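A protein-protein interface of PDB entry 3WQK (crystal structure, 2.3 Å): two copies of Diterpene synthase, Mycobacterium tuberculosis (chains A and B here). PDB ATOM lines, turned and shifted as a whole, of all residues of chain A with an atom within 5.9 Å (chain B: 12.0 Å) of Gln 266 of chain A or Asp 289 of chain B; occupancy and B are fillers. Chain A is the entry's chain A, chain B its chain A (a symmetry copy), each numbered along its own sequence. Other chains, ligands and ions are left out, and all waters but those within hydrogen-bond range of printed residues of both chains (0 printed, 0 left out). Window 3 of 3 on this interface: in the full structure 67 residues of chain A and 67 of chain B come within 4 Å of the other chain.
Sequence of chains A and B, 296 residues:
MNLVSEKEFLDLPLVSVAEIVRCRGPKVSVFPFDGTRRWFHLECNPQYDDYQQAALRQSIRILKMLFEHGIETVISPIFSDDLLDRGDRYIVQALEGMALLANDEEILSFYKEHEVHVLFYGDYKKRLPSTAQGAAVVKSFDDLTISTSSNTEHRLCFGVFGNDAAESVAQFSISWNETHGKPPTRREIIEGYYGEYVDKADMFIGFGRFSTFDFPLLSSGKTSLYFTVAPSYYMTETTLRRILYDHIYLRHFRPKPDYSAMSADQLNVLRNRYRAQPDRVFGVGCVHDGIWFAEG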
ATOM      1  N   PRO A 257       7.894  25.214  -8.723  1.00  0.00           N
ATOM      2  CA  PRO A 257       6.656  25.912  -8.361  1.00  0.00           C
ATOM      3  C   PRO A 257       6.828  27.087  -7.397  1.00  0.00           C
ATOM      4  O   PRO A 257       7.547  26.988  -6.400  1.00  0.00           O
ATOM      5  CB  PRO A 257       5.812  24.798  -7.757  1.00  0.00           C
ATOM      6  CG  PRO A 257       6.840  24.000  -7.023  1.00  0.00           C
ATOM      7  CD  PRO A 257       7.983  23.916  -8.026  1.00  0.00           C
ATOM      8  N   TYR A 259       4.663  29.058  -5.017  1.00  0.00           N
ATOM      9  CA  TYR A 259       3.387  29.125  -4.313  1.00  0.00           C
ATOM     10  C   TYR A 259       2.848  30.543  -4.151  1.00  0.00           C
ATOM     11  O   TYR A 259       1.686  30.812  -4.460  1.00  0.00           O
ATOM     12  CB  TYR A 259       3.515  28.463  -2.935  1.00  0.00           C
ATOM     13  CG  TYR A 259       3.921  26.999  -2.973  1.00  0.00           C
ATOM     14  CD1 TYR A 259       4.048  26.262  -1.795  1.00  0.00           C
ATOM     15  CD2 TYR A 259       4.188  26.353  -4.184  1.00  0.00           C
ATOM     16  CE1 TYR A 259       4.432  24.920  -1.819  1.00  0.00           C
ATOM     17  CE2 TYR A 259       4.574  25.012  -4.219  1.00  0.00           C
ATOM     18  CZ  TYR A 259       4.695  24.303  -3.034  1.00  0.00           C
ATOM     19  OH  TYR A 259       5.086  22.983  -3.068  1.00  0.00           O
ATOM     20  N   ALA A 261       3.084  33.011  -5.867  1.00  0.00           N
ATOM     21  CA  ALA A 261       2.587  33.578  -7.119  1.00  0.00           C
ATOM     22  C   ALA A 261       1.252  33.003  -7.587  1.00  0.00           C
ATOM     23  O   ALA A 261       0.655  33.511  -8.536  1.00  0.00           O
ATOM     24  CB  ALA A 261       3.634  33.404  -8.215  1.00  0.00           C
ATOM     25  N   MET A 262       0.783  31.950  -6.924  1.00  0.00           N
ATOM     26  CA  MET A 262      -0.480  31.318  -7.301  1.00  0.00           C
ATOM     27  C   MET A 262      -1.701  31.936  -6.622  1.00  0.00           C
ATOM     28  O   MET A 262      -1.635  32.371  -5.472  1.00  0.00           O
ATOM     29  CB  MET A 262      -0.440  29.817  -6.989  1.00  0.00           C
ATOM     30  CG  MET A 262       0.554  29.021  -7.820  1.00  0.00           C
ATOM     31  SD  MET A 262       0.337  27.236  -7.601  1.00  0.00           S
ATOM     32  CE  MET A 262       1.126  26.980  -6.000  1.00  0.00           C
ATOM     33  N   SER A 263      -2.819  31.956  -7.343  1.00  0.00           N
ATOM     34  CA  SER A 263      -4.059  32.511  -6.818  1.00  0.00           C
ATOM     35  C   SER A 263      -4.541  31.688  -5.631  1.00  0.00           C
ATOM     36  O   SER A 263      -4.058  30.581  -5.391  1.00  0.00           O
ATOM     37  CB  SER A 263      -5.140  32.518  -7.901  1.00  0.00           C
ATOM     38  OG  SER A 263      -5.516  31.199  -8.254  1.00  0.00           O
ATOM     39  N   ALA A 264      -5.496  32.232  -4.888  1.00  0.00           N
ATOM     40  CA  ALA A 264      -6.031  31.531  -3.732  1.00  0.00           C
ATOM     41  C   ALA A 264      -6.826  30.304  -4.183  1.00  0.00           C
ATOM     42  O   ALA A 264      -6.977  29.341  -3.427  1.00  0.00           O
ATOM     43  CB  ALA A 264      -6.917  32.467  -2.916  1.00  0.00           C
ATOM     44  N   ASP A 265      -7.329  30.337  -5.415  1.00  0.00           N
ATOM     45  CA  ASP A 265      -8.102  29.212  -5.928  1.00  0.00           C
ATOM     46  C   ASP A 265      -7.177  28.070  -6.329  1.00  0.00           C
ATOM     47  O   ASP A 265      -7.478  26.902  -6.080  1.00  0.00           O
ATOM     48  CB  ASP A 265      -8.949  29.632  -7.132  1.00  0.00           C
ATOM     49  CG  ASP A 265      -9.997  28.592  -7.490  1.00  0.00           C
ATOM     50  OD1 ASP A 265     -10.898  28.348  -6.659  1.00  0.00           O
ATOM     51  OD2 ASP A 265      -9.919  28.012  -8.594  1.00  0.00           O
ATOM     52  N   GLN A 266      -6.055  28.414  -6.955  1.00  0.00           N
ATOM     53  CA  GLN A 266      -5.078  27.414  -7.371  1.00  0.00           C
ATOM     54  C   GLN A 266      -4.618  26.615  -6.157  1.00  0.00           C
ATOM     55  O   GLN A 266      -4.646  25.384  -6.165  1.00  0.00           O
ATOM     56  CB  GLN A 266      -3.866  28.083  -8.029  1.00  0.00           C
ATOM     57  CG  GLN A 266      -4.153  28.745  -9.364  1.00  0.00           C
ATOM     58  CD  GLN A 266      -2.919  29.406  -9.961  1.00  0.00           C
ATOM     59  OE1 GLN A 266      -2.265  30.220  -9.311  1.00  0.00           O
ATOM     60  NE2 GLN A 266      -2.600  29.062 -11.207  1.00  0.00           N
ATOM     61  N   LEU A 267      -4.194  27.321  -5.113  1.00  0.00           N
ATOM     62  CA  LEU A 267      -3.739  26.659  -3.900  1.00  0.00           C
ATOM     63  C   LEU A 267      -4.856  25.767  -3.387  1.00  0.00           C
ATOM     64  O   LEU A 267      -4.612  24.669  -2.881  1.00  0.00           O
ATOM     65  CB  LEU A 267      -3.381  27.681  -2.815  1.00  0.00           C
ATOM     66  CG  LEU A 267      -2.417  28.834  -3.113  1.00  0.00           C
ATOM     67  CD1 LEU A 267      -1.928  29.396  -1.783  1.00  0.00           C
ATOM     68  CD2 LEU A 267      -1.228  28.359  -3.938  1.00  0.00           C
ATOM     69  N   ASN A 268      -6.085  26.248  -3.524  1.00  0.00           N
ATOM     70  CA  ASN A 268      -7.252  25.507  -3.067  1.00  0.00           C
ATOM     71  C   ASN A 268      -7.475  24.234  -3.894  1.00  0.00           C
ATOM     72  O   ASN A 268      -7.815  23.182  -3.353  1.00  0.00           O
ATOM     73  CB  ASN A 268      -8.487  26.405  -3.137  1.00  0.00           C
ATOM     74  CG  ASN A 268      -9.549  25.999  -2.146  1.00  0.00           C
ATOM     75  OD1 ASN A 268      -9.329  26.045  -0.933  1.00  0.00           O
ATOM     76  ND2 ASN A 268     -10.712  25.593  -2.653  1.00  0.00           N
ATOM     77  N   VAL A 269      -7.292  24.343  -5.206  1.00  0.00           N
ATOM     78  CA  VAL A 269      -7.452  23.201  -6.102  1.00  0.00           C
ATOM     79  C   VAL A 269      -6.348  22.183  -5.805  1.00  0.00           C
ATOM     80  O   VAL A 269      -6.580  20.977  -5.833  1.00  0.00           O
ATOM     81  CB  VAL A 269      -7.360  23.634  -7.592  1.00  0.00           C
ATOM     82  CG1 VAL A 269      -7.202  22.411  -8.486  1.00  0.00           C
ATOM     83  CG2 VAL A 269      -8.610  24.407  -7.985  1.00  0.00           C
ATOM     84  N   LEU A 270      -5.152  22.685  -5.517  1.00  0.00           N
ATOM     85  CA  LEU A 270      -4.024  21.824  -5.203  1.00  0.00           C
ATOM     86  C   LEU A 270      -4.295  21.118  -3.884  1.00  0.00           C
ATOM     87  O   LEU A 270      -4.080  19.911  -3.758  1.00  0.00           O
ATOM     88  CB  LEU A 270      -2.742  22.647  -5.105  1.00  0.00           C
ATOM     89  CG  LEU A 270      -1.437  21.875  -4.891  1.00  0.00           C
ATOM     90  CD1 LEU A 270      -1.255  20.829  -5.988  1.00  0.00           C
ATOM     91  CD2 LEU A 270      -0.280  22.861  -4.896  1.00  0.00           C
ATOM     92  N   ARG A 271      -4.773  21.872  -2.900  1.00  0.00           N
ATOM     93  CA  ARG A 271      -5.081  21.292  -1.601  1.00  0.00           C
ATOM     94  C   ARG A 271      -6.115  20.179  -1.734  1.00  0.00           C
ATOM     95  O   ARG A 271      -6.044  19.175  -1.029  1.00  0.00           O
ATOM     96  CB  ARG A 271      -5.588  22.370  -0.634  1.00  0.00           C
ATOM     97  CG  ARG A 271      -6.306  21.806   0.597  1.00  0.00           C
ATOM     98  CD  ARG A 271      -6.385  22.794   1.769  1.00  0.00           C
ATOM     99  NE  ARG A 271      -6.899  24.109   1.390  1.00  0.00           N
ATOM    100  CZ  ARG A 271      -6.156  25.086   0.875  1.00  0.00           C
ATOM    101  NH1 ARG A 271      -4.858  24.905   0.675  1.00  0.00           N
ATOM    102  NH2 ARG A 271      -6.711  26.250   0.562  1.00  0.00           N
ATOM    103  N   ARG B  37       7.525  22.306   3.292  1.00  0.00           N
ATOM    104  CA  ARG B  37       7.181  23.637   2.795  1.00  0.00           C
ATOM    105  C   ARG B  37       5.814  23.637   2.126  1.00  0.00           C
ATOM    106  O   ARG B  37       4.992  24.518   2.370  1.00  0.00           O
ATOM    107  CB  ARG B  37       8.236  24.129   1.801  1.00  0.00           C
ATOM    108  CG  ARG B  37       9.632  24.278   2.388  1.00  0.00           C
ATOM    109  CD  ARG B  37      10.580  24.884   1.369  1.00  0.00           C
ATOM    110  NE  ARG B  37      10.081  26.169   0.889  1.00  0.00           N
ATOM    111  CZ  ARG B  37      10.705  26.935   0.000  1.00  0.00           C
ATOM    112  NH1 ARG B  37      11.864  26.545  -0.519  1.00  0.00           N
ATOM    113  NH2 ARG B  37      10.166  28.091  -0.371  1.00  0.00           N
ATOM    114  N   ARG B  38       5.582  22.640   1.279  1.00  0.00           N
ATOM    115  CA  ARG B  38       4.318  22.503   0.570  1.00  0.00           C
ATOM    116  C   ARG B  38       3.172  22.403   1.574  1.00  0.00           C
ATOM    117  O   ARG B  38       2.177  23.123   1.476  1.00  0.00           O
ATOM    118  CB  ARG B  38       4.357  21.250  -0.304  1.00  0.00           C
ATOM    119  CG  ARG B  38       3.220  21.128  -1.298  1.00  0.00           C
ATOM    120  CD  ARG B  38       3.420  19.903  -2.170  1.00  0.00           C
ATOM    121  NE  ARG B  38       4.775  19.851  -2.717  1.00  0.00           N
ATOM    122  CZ  ARG B  38       5.207  18.921  -3.562  1.00  0.00           C
ATOM    123  NH1 ARG B  38       4.389  17.958  -3.964  1.00  0.00           N
ATOM    124  NH2 ARG B  38       6.455  18.953  -4.011  1.00  0.00           N
ATOM    125  N   HIS B  41       2.314  25.833   3.075  1.00  0.00           N
ATOM    126  CA  HIS B  41       1.541  26.747   2.249  1.00  0.00           C
ATOM    127  C   HIS B  41       0.179  26.177   1.870  1.00  0.00           C
ATOM    128  O   HIS B  41      -0.492  26.704   0.985  1.00  0.00           O
ATOM    129  CB  HIS B  41       2.334  27.085   0.988  1.00  0.00           C
ATOM    130  CG  HIS B  41       3.649  27.744   1.269  1.00  0.00           C
ATOM    131  ND1 HIS B  41       3.747  29.035   1.743  1.00  0.00           N
ATOM    132  CD2 HIS B  41       4.918  27.279   1.178  1.00  0.00           C
ATOM    133  CE1 HIS B  41       5.020  29.336   1.932  1.00  0.00           C
ATOM    134  NE2 HIS B  41       5.750  28.288   1.596  1.00  0.00           N
ATOM    135  N   LEU B  42      -0.232  25.106   2.542  1.00  0.00           N
ATOM    136  CA  LEU B  42      -1.516  24.477   2.251  1.00  0.00           C
ATOM    137  C   LEU B  42      -2.379  24.222   3.483  1.00  0.00           C
ATOM    138  O   LEU B  42      -3.601  24.128   3.379  1.00  0.00           O
ATOM    139  CB  LEU B  42      -1.301  23.151   1.516  1.00  0.00           C
ATOM    140  CG  LEU B  42      -0.733  23.191   0.097  1.00  0.00           C
ATOM    141  CD1 LEU B  42      -0.481  21.773  -0.387  1.00  0.00           C
ATOM    142  CD2 LEU B  42      -1.707  23.909  -0.828  1.00  0.00           C
ATOM    143  N   GLU B  43      -1.750  24.107   4.647  1.00  0.00           N
ATOM    144  CA  GLU B  43      -2.498  23.838   5.869  1.00  0.00           C
ATOM    145  C   GLU B  43      -2.372  24.923   6.930  1.00  0.00           C
ATOM    146  O   GLU B  43      -3.275  25.103   7.747  1.00  0.00           O
ATOM    147  CB  GLU B  43      -2.065  22.496   6.461  1.00  0.00           C
ATOM    148  CG  GLU B  43      -2.302  21.322   5.536  1.00  0.00           C
ATOM    149  CD  GLU B  43      -3.730  21.264   5.041  1.00  0.00           C
ATOM    150  OE1 GLU B  43      -4.646  21.163   5.885  1.00  0.00           O
ATOM    151  OE2 GLU B  43      -3.936  21.325   3.810  1.00  0.00           O
ATOM    152  N   ASN B  45      -2.229  28.710   7.283  1.00  0.00           N
ATOM    153  CA  ASN B  45      -2.422  30.053   6.742  1.00  0.00           C
ATOM    154  C   ASN B  45      -3.906  30.416   6.764  1.00  0.00           C
ATOM    155  O   ASN B  45      -4.351  31.318   6.053  1.00  0.00           O
ATOM    156  CB  ASN B  45      -1.886  30.153   5.305  1.00  0.00           C
ATOM    157  CG  ASN B  45      -2.619  29.239   4.332  1.00  0.00           C
ATOM    158  OD1 ASN B  45      -2.424  29.328   3.118  1.00  0.00           O
ATOM    159  ND2 ASN B  45      -3.458  28.353   4.858  1.00  0.00           N
ATOM    160  N   PHE B 207       6.603   9.942  -0.416  1.00  0.00           N
ATOM    161  CA  PHE B 207       5.398  10.586  -0.921  1.00  0.00           C
ATOM    162  C   PHE B 207       5.702  11.160  -2.295  1.00  0.00           C
ATOM    163  O   PHE B 207       6.859  11.422  -2.624  1.00  0.00           O
ATOM    164  CB  PHE B 207       4.954  11.704   0.046  1.00  0.00           C
ATOM    165  CG  PHE B 207       5.352  13.088  -0.390  1.00  0.00           C
ATOM    166  CD1 PHE B 207       4.551  13.811  -1.276  1.00  0.00           C
ATOM    167  CD2 PHE B 207       6.546  13.652   0.046  1.00  0.00           C
ATOM    168  CE1 PHE B 207       4.938  15.079  -1.727  1.00  0.00           C
ATOM    169  CE2 PHE B 207       6.945  14.919  -0.396  1.00  0.00           C
ATOM    170  CZ  PHE B 207       6.138  15.633  -1.286  1.00  0.00           C
ATOM    171  N   ARG B 209       6.632  11.663  -6.004  1.00  0.00           N
ATOM    172  CA  ARG B 209       7.527  10.965  -6.923  1.00  0.00           C
ATOM    173  C   ARG B 209       8.117   9.695  -6.298  1.00  0.00           C
ATOM    174  O   ARG B 209       8.632   9.729  -5.182  1.00  0.00           O
ATOM    175  CB  ARG B 209       8.655  11.914  -7.365  1.00  0.00           C
ATOM    176  CG  ARG B 209       8.212  12.923  -8.429  1.00  0.00           C
ATOM    177  CD  ARG B 209       9.253  14.017  -8.644  1.00  0.00           C
ATOM    178  NE  ARG B 209       9.515  14.720  -7.393  1.00  0.00           N
ATOM    179  CZ  ARG B 209      10.387  15.713  -7.261  1.00  0.00           C
ATOM    180  NH1 ARG B 209      11.081  16.127  -8.317  1.00  0.00           N
ATOM    181  NH2 ARG B 209      10.582  16.277  -6.074  1.00  0.00           N
ATOM    182  N   TYR B 234       0.894  14.687   6.335  1.00  0.00           N
ATOM    183  CA  TYR B 234      -0.517  14.362   6.138  1.00  0.00           C
ATOM    184  C   TYR B 234      -0.863  12.944   6.593  1.00  0.00           C
ATOM    185  O   TYR B 234      -2.035  12.587   6.693  1.00  0.00           O
ATOM    186  CB  TYR B 234      -0.893  14.506   4.662  1.00  0.00           C
ATOM    187  CG  TYR B 234      -1.178  15.917   4.195  1.00  0.00           C
ATOM    188  CD1 TYR B 234      -2.268  16.634   4.693  1.00  0.00           C
ATOM    189  CD2 TYR B 234      -0.396  16.512   3.207  1.00  0.00           C
ATOM    190  CE1 TYR B 234      -2.573  17.911   4.209  1.00  0.00           C
ATOM    191  CE2 TYR B 234      -0.689  17.782   2.718  1.00  0.00           C
ATOM    192  CZ  TYR B 234      -1.778  18.476   3.217  1.00  0.00           C
ATOM    193  OH  TYR B 234      -2.076  19.724   2.708  1.00  0.00           O
ATOM    194  N   GLY B 285       3.778   9.602 -14.040  1.00  0.00           N
ATOM    195  CA  GLY B 285       2.813  10.552 -13.524  1.00  0.00           C
ATOM    196  C   GLY B 285       2.388  11.639 -14.489  1.00  0.00           C
ATOM    197  O   GLY B 285       2.464  11.495 -15.713  1.00  0.00           O
ATOM    198  N   CYS B 286       1.925  12.738 -13.911  1.00  0.00           N
ATOM    199  CA  CYS B 286       1.479  13.896 -14.663  1.00  0.00           C
ATOM    200  C   CYS B 286       1.787  15.098 -13.782  1.00  0.00           C
ATOM    201  O   CYS B 286       1.929  14.955 -12.563  1.00  0.00           O
ATOM    202  CB  CYS B 286      -0.019  13.792 -14.934  1.00  0.00           C
ATOM    203  SG  CYS B 286      -0.963  13.548 -13.440  1.00  0.00           S
ATOM    204  N   VAL B 287       1.896  16.279 -14.379  1.00  0.00           N
ATOM    205  CA  VAL B 287       2.220  17.461 -13.597  1.00  0.00           C
ATOM    206  C   VAL B 287       1.108  18.506 -13.534  1.00  0.00           C
ATOM    207  O   VAL B 287       0.466  18.809 -14.542  1.00  0.00           O
ATOM    208  CB  VAL B 287       3.509  18.129 -14.128  1.00  0.00           C
ATOM    209  CG1 VAL B 287       3.828  19.387 -13.316  1.00  0.00           C
ATOM    210  CG2 VAL B 287       4.665  17.146 -14.043  1.00  0.00           C
ATOM    211  N   HIS B 288       0.885  19.036 -12.332  1.00  0.00           N
ATOM    212  CA  HIS B 288      -0.119  20.071 -12.091  1.00  0.00           C
ATOM    213  C   HIS B 288       0.545  21.129 -11.233  1.00  0.00           C
ATOM    214  O   HIS B 288       1.046  20.821 -10.145  1.00  0.00           O
ATOM    215  CB  HIS B 288      -1.329  19.503 -11.344  1.00  0.00           C
ATOM    216  CG  HIS B 288      -2.059  18.438 -12.101  1.00  0.00           C
ATOM    217  ND1 HIS B 288      -2.746  18.693 -13.266  1.00  0.00           N
ATOM    218  CD2 HIS B 288      -2.184  17.108 -11.872  1.00  0.00           C
ATOM    219  CE1 HIS B 288      -3.264  17.567 -13.725  1.00  0.00           C
ATOM    220  NE2 HIS B 288      -2.938  16.590 -12.898  1.00  0.00           N
ATOM    221  N   ASP B 289       0.559  22.369 -11.715  1.00  0.00           N
ATOM    222  CA  ASP B 289       1.175  23.456 -10.966  1.00  0.00           C
ATOM    223  C   ASP B 289       2.607  23.125 -10.597  1.00  0.00           C
ATOM    224  O   ASP B 289       3.064  23.452  -9.498  1.00  0.00           O
ATOM    225  CB  ASP B 289       0.384  23.745  -9.687  1.00  0.00           C
ATOM    226  CG  ASP B 289      -0.904  24.487  -9.959  1.00  0.00           C
ATOM    227  OD1 ASP B 289      -1.441  24.355 -11.081  1.00  0.00           O
ATOM    228  OD2 ASP B 289      -1.385  25.193  -9.045  1.00  0.00           O
ATOM    229  N   GLY B 290       3.308  22.470 -11.514  1.00  0.00           N
ATOM    230  CA  GLY B 290       4.696  22.120 -11.274  1.00  0.00           C
ATOM    231  C   GLY B 290       4.905  20.961 -10.320  1.00  0.00           C
ATOM    232  O   GLY B 290       6.040  20.611  -9.994  1.00  0.00           O
ATOM    233  N   ILE B 291       3.809  20.361  -9.873  1.00  0.00           N
ATOM    234  CA  ILE B 291       3.873  19.243  -8.949  1.00  0.00           C
ATOM    235  C   ILE B 291       3.468  17.932  -9.628  1.00  0.00           C
ATOM    236  O   ILE B 291       2.384  17.811 -10.206  1.00  0.00           O
ATOM    237  CB  ILE B 291       2.961  19.494  -7.734  1.00  0.00           C
ATOM    238  CG1 ILE B 291       3.451  20.732  -6.978  1.00  0.00           C
ATOM    239  CG2 ILE B 291       2.934  18.266  -6.828  1.00  0.00           C
ATOM    240  CD1 ILE B 291       2.547  21.141  -5.832  1.00  0.00           C
ATOM    241  N   TRP B 292       4.360  16.955  -9.532  1.00  0.00           N
ATOM    242  CA  TRP B 292       4.176  15.633 -10.105  1.00  0.00           C
ATOM    243  C   TRP B 292       3.198  14.796  -9.270  1.00  0.00           C
ATOM    244  O   TRP B 292       3.257  14.805  -8.041  1.00  0.00           O
ATOM    245  CB  TRP B 292       5.544  14.941 -10.162  1.00  0.00           C
ATOM    246  CG  TRP B 292       5.561  13.596 -10.807  1.00  0.00           C
ATOM    247  CD1 TRP B 292       5.908  13.310 -12.092  1.00  0.00           C
ATOM    248  CD2 TRP B 292       5.246  12.343 -10.186  1.00  0.00           C
ATOM    249  NE1 TRP B 292       5.833  11.951 -12.316  1.00  0.00           N
ATOM    250  CE2 TRP B 292       5.429  11.336 -11.159  1.00  0.00           C
ATOM    251  CE3 TRP B 292       4.827  11.975  -8.897  1.00  0.00           C
ATOM    252  CZ2 TRP B 292       5.210   9.978 -10.886  1.00  0.00           C
ATOM    253  CZ3 TRP B 292       4.609  10.633  -8.625  1.00  0.00           C
ATOM    254  CH2 TRP B 292       4.801   9.651  -9.616  1.00  0.00           C
ATOM    255  N   PHE B 293       2.290  14.093  -9.938  1.00  0.00           N
ATOM    256  CA  PHE B 293       1.331  13.216  -9.264  1.00  0.00           C
ATOM    257  C   PHE B 293       1.352  11.889 -10.009  1.00  0.00           C
ATOM    258  O   PHE B 293       1.331  11.866 -11.238  1.00  0.00           O
ATOM    259  CB  PHE B 293      -0.106  13.765  -9.309  1.00  0.00           C
ATOM    260  CG  PHE B 293      -0.334  14.967  -8.441  1.00  0.00           C
ATOM    261  CD1 PHE B 293       0.134  16.221  -8.823  1.00  0.00           C
ATOM    262  CD2 PHE B 293      -1.020  14.846  -7.237  1.00  0.00           C
ATOM    263  CE1 PHE B 293      -0.082  17.336  -8.018  1.00  0.00           C
ATOM    264  CE2 PHE B 293      -1.240  15.955  -6.427  1.00  0.00           C
ATOM    265  CZ  PHE B 293      -0.769  17.200  -6.817  1.00  0.00           C
ATOM    266  N   ALA B 294       1.396  10.789  -9.266  1.00  0.00           N
ATOM    267  CA  ALA B 294       1.408   9.461  -9.869  1.00  0.00           C
ATOM    268  C   ALA B 294       0.047   9.174 -10.509  1.00  0.00           C
ATOM    269  O   ALA B 294      -0.985   9.567  -9.960  1.00  0.00           O
ATOM    270  CB  ALA B 294       1.715   8.412  -8.799  1.00  0.00           C
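Of chain B, only Asp 289 (3.9 Å) comes within 4 Å of Gln 266 of chain A.
Of chain A, only Pro 257 (3.5 Å), Met 262 (3.0 Å) and Gln 266 (3.9 Å) come within 4 Å of Asp 289 of chain B.
Pro 257 of chain A touches just one residue of chain B: Asp 289.
Ala 261 of chain A touches none of the printed residues of chain B.
Met 262 of chain A touches one residue of chain B.
Ser 263 of chain A touches none of the printed residues of chain B.
No residue of chain B comes within 4 Å of Ala 264 of chain A.
No residue of chain B comes within 4 Å of Asp 265 of chain A.
Leu 267 of chain A touches just one residue of chain B: Leu 42 (3.6 Å).
No residue of chain B comes within 4 Å of Asn 268 of chain A.
No residue of chain B comes within 4 Å of Val 269 of chain A.
Printed residues of chain A within 4 Å of Ile 291 of chain B: Leu 270.
Of the printed residues of chain B, Tyr 259 of chain A touches Arg 38 (3.2 Å) and His 41 (3.3 Å).
The nearest residue of chain B that does not touch Gln 266 of chain A is Leu 42 of chain B (6.3 Å).
The nearest printed residue of chain A that does not touch Ile 291 of chain B is Tyr 259 of chain A (4.2 Å).
Among the printed residues, pairs that only touch across the chains: Tyr 259 of chain A with His 41 of chain B, Leu 270 of chain A with Ile 291 of chain B, Arg 271 of chain A with Glu 43 of chain B, Pro 257 of chain A with Asp 289 of chain B, Leu 267 of chain A with Leu 42 of chain B, Leu 270 of chain A with Phe 293 of chain B and Gln 266 of chain A with Asp 289 of chain B.
SD of Met 262 of chain A lies close to OD2 of Asp 289 of chain B, at 3.0 Å.
The side-chain hydroxyl (OH) of Tyr 259 of chain A sits at hydrogen-bond distance from the guanidinium group (NE) of Arg 38 of chain B (3.2 Å).
The guanidinium group (NH1) of Arg 271 of chain A lies within hydrogen-bond range of the backbone carbonyl oxygen (O) of Leu 42 of chain B (3.1 Å).
Hydrophobic or aromatic side chains of chain A that line the printed part of chain B: Pro 257, Tyr 259, Met 262 and Leu 270.
Printed residues of chain B that touch a printed residue of chain A: Arg 38, His 41, Leu 42, Glu 43, Asp 289, Ile 291 and Phe 293.
Among the printed residues, 10 pairs touch across the chains.
No position is printed for both chains.
OE1 of Gln 266 of chain A is in hydrogen-bond range of N of Ser 263 of chain A.
The side-chain carboxylate (OE2) of Glu 43 of chain B is in hydrogen-bond range of the side-chain hydroxyl (OH) of Tyr 234 of chain B (2.7 Å).
The backbone NH (N) of Phe 293 of chain B lies within hydrogen-bond range of the backbone carbonyl oxygen (O) of Cys 286 of chain B (2.8 Å).
The side-chain amide oxygen (OD1) of Asn 268 of chain A lies within hydrogen-bond range of the guanidinium group (NH2) of Arg 271 of chain A (3.0 Å).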
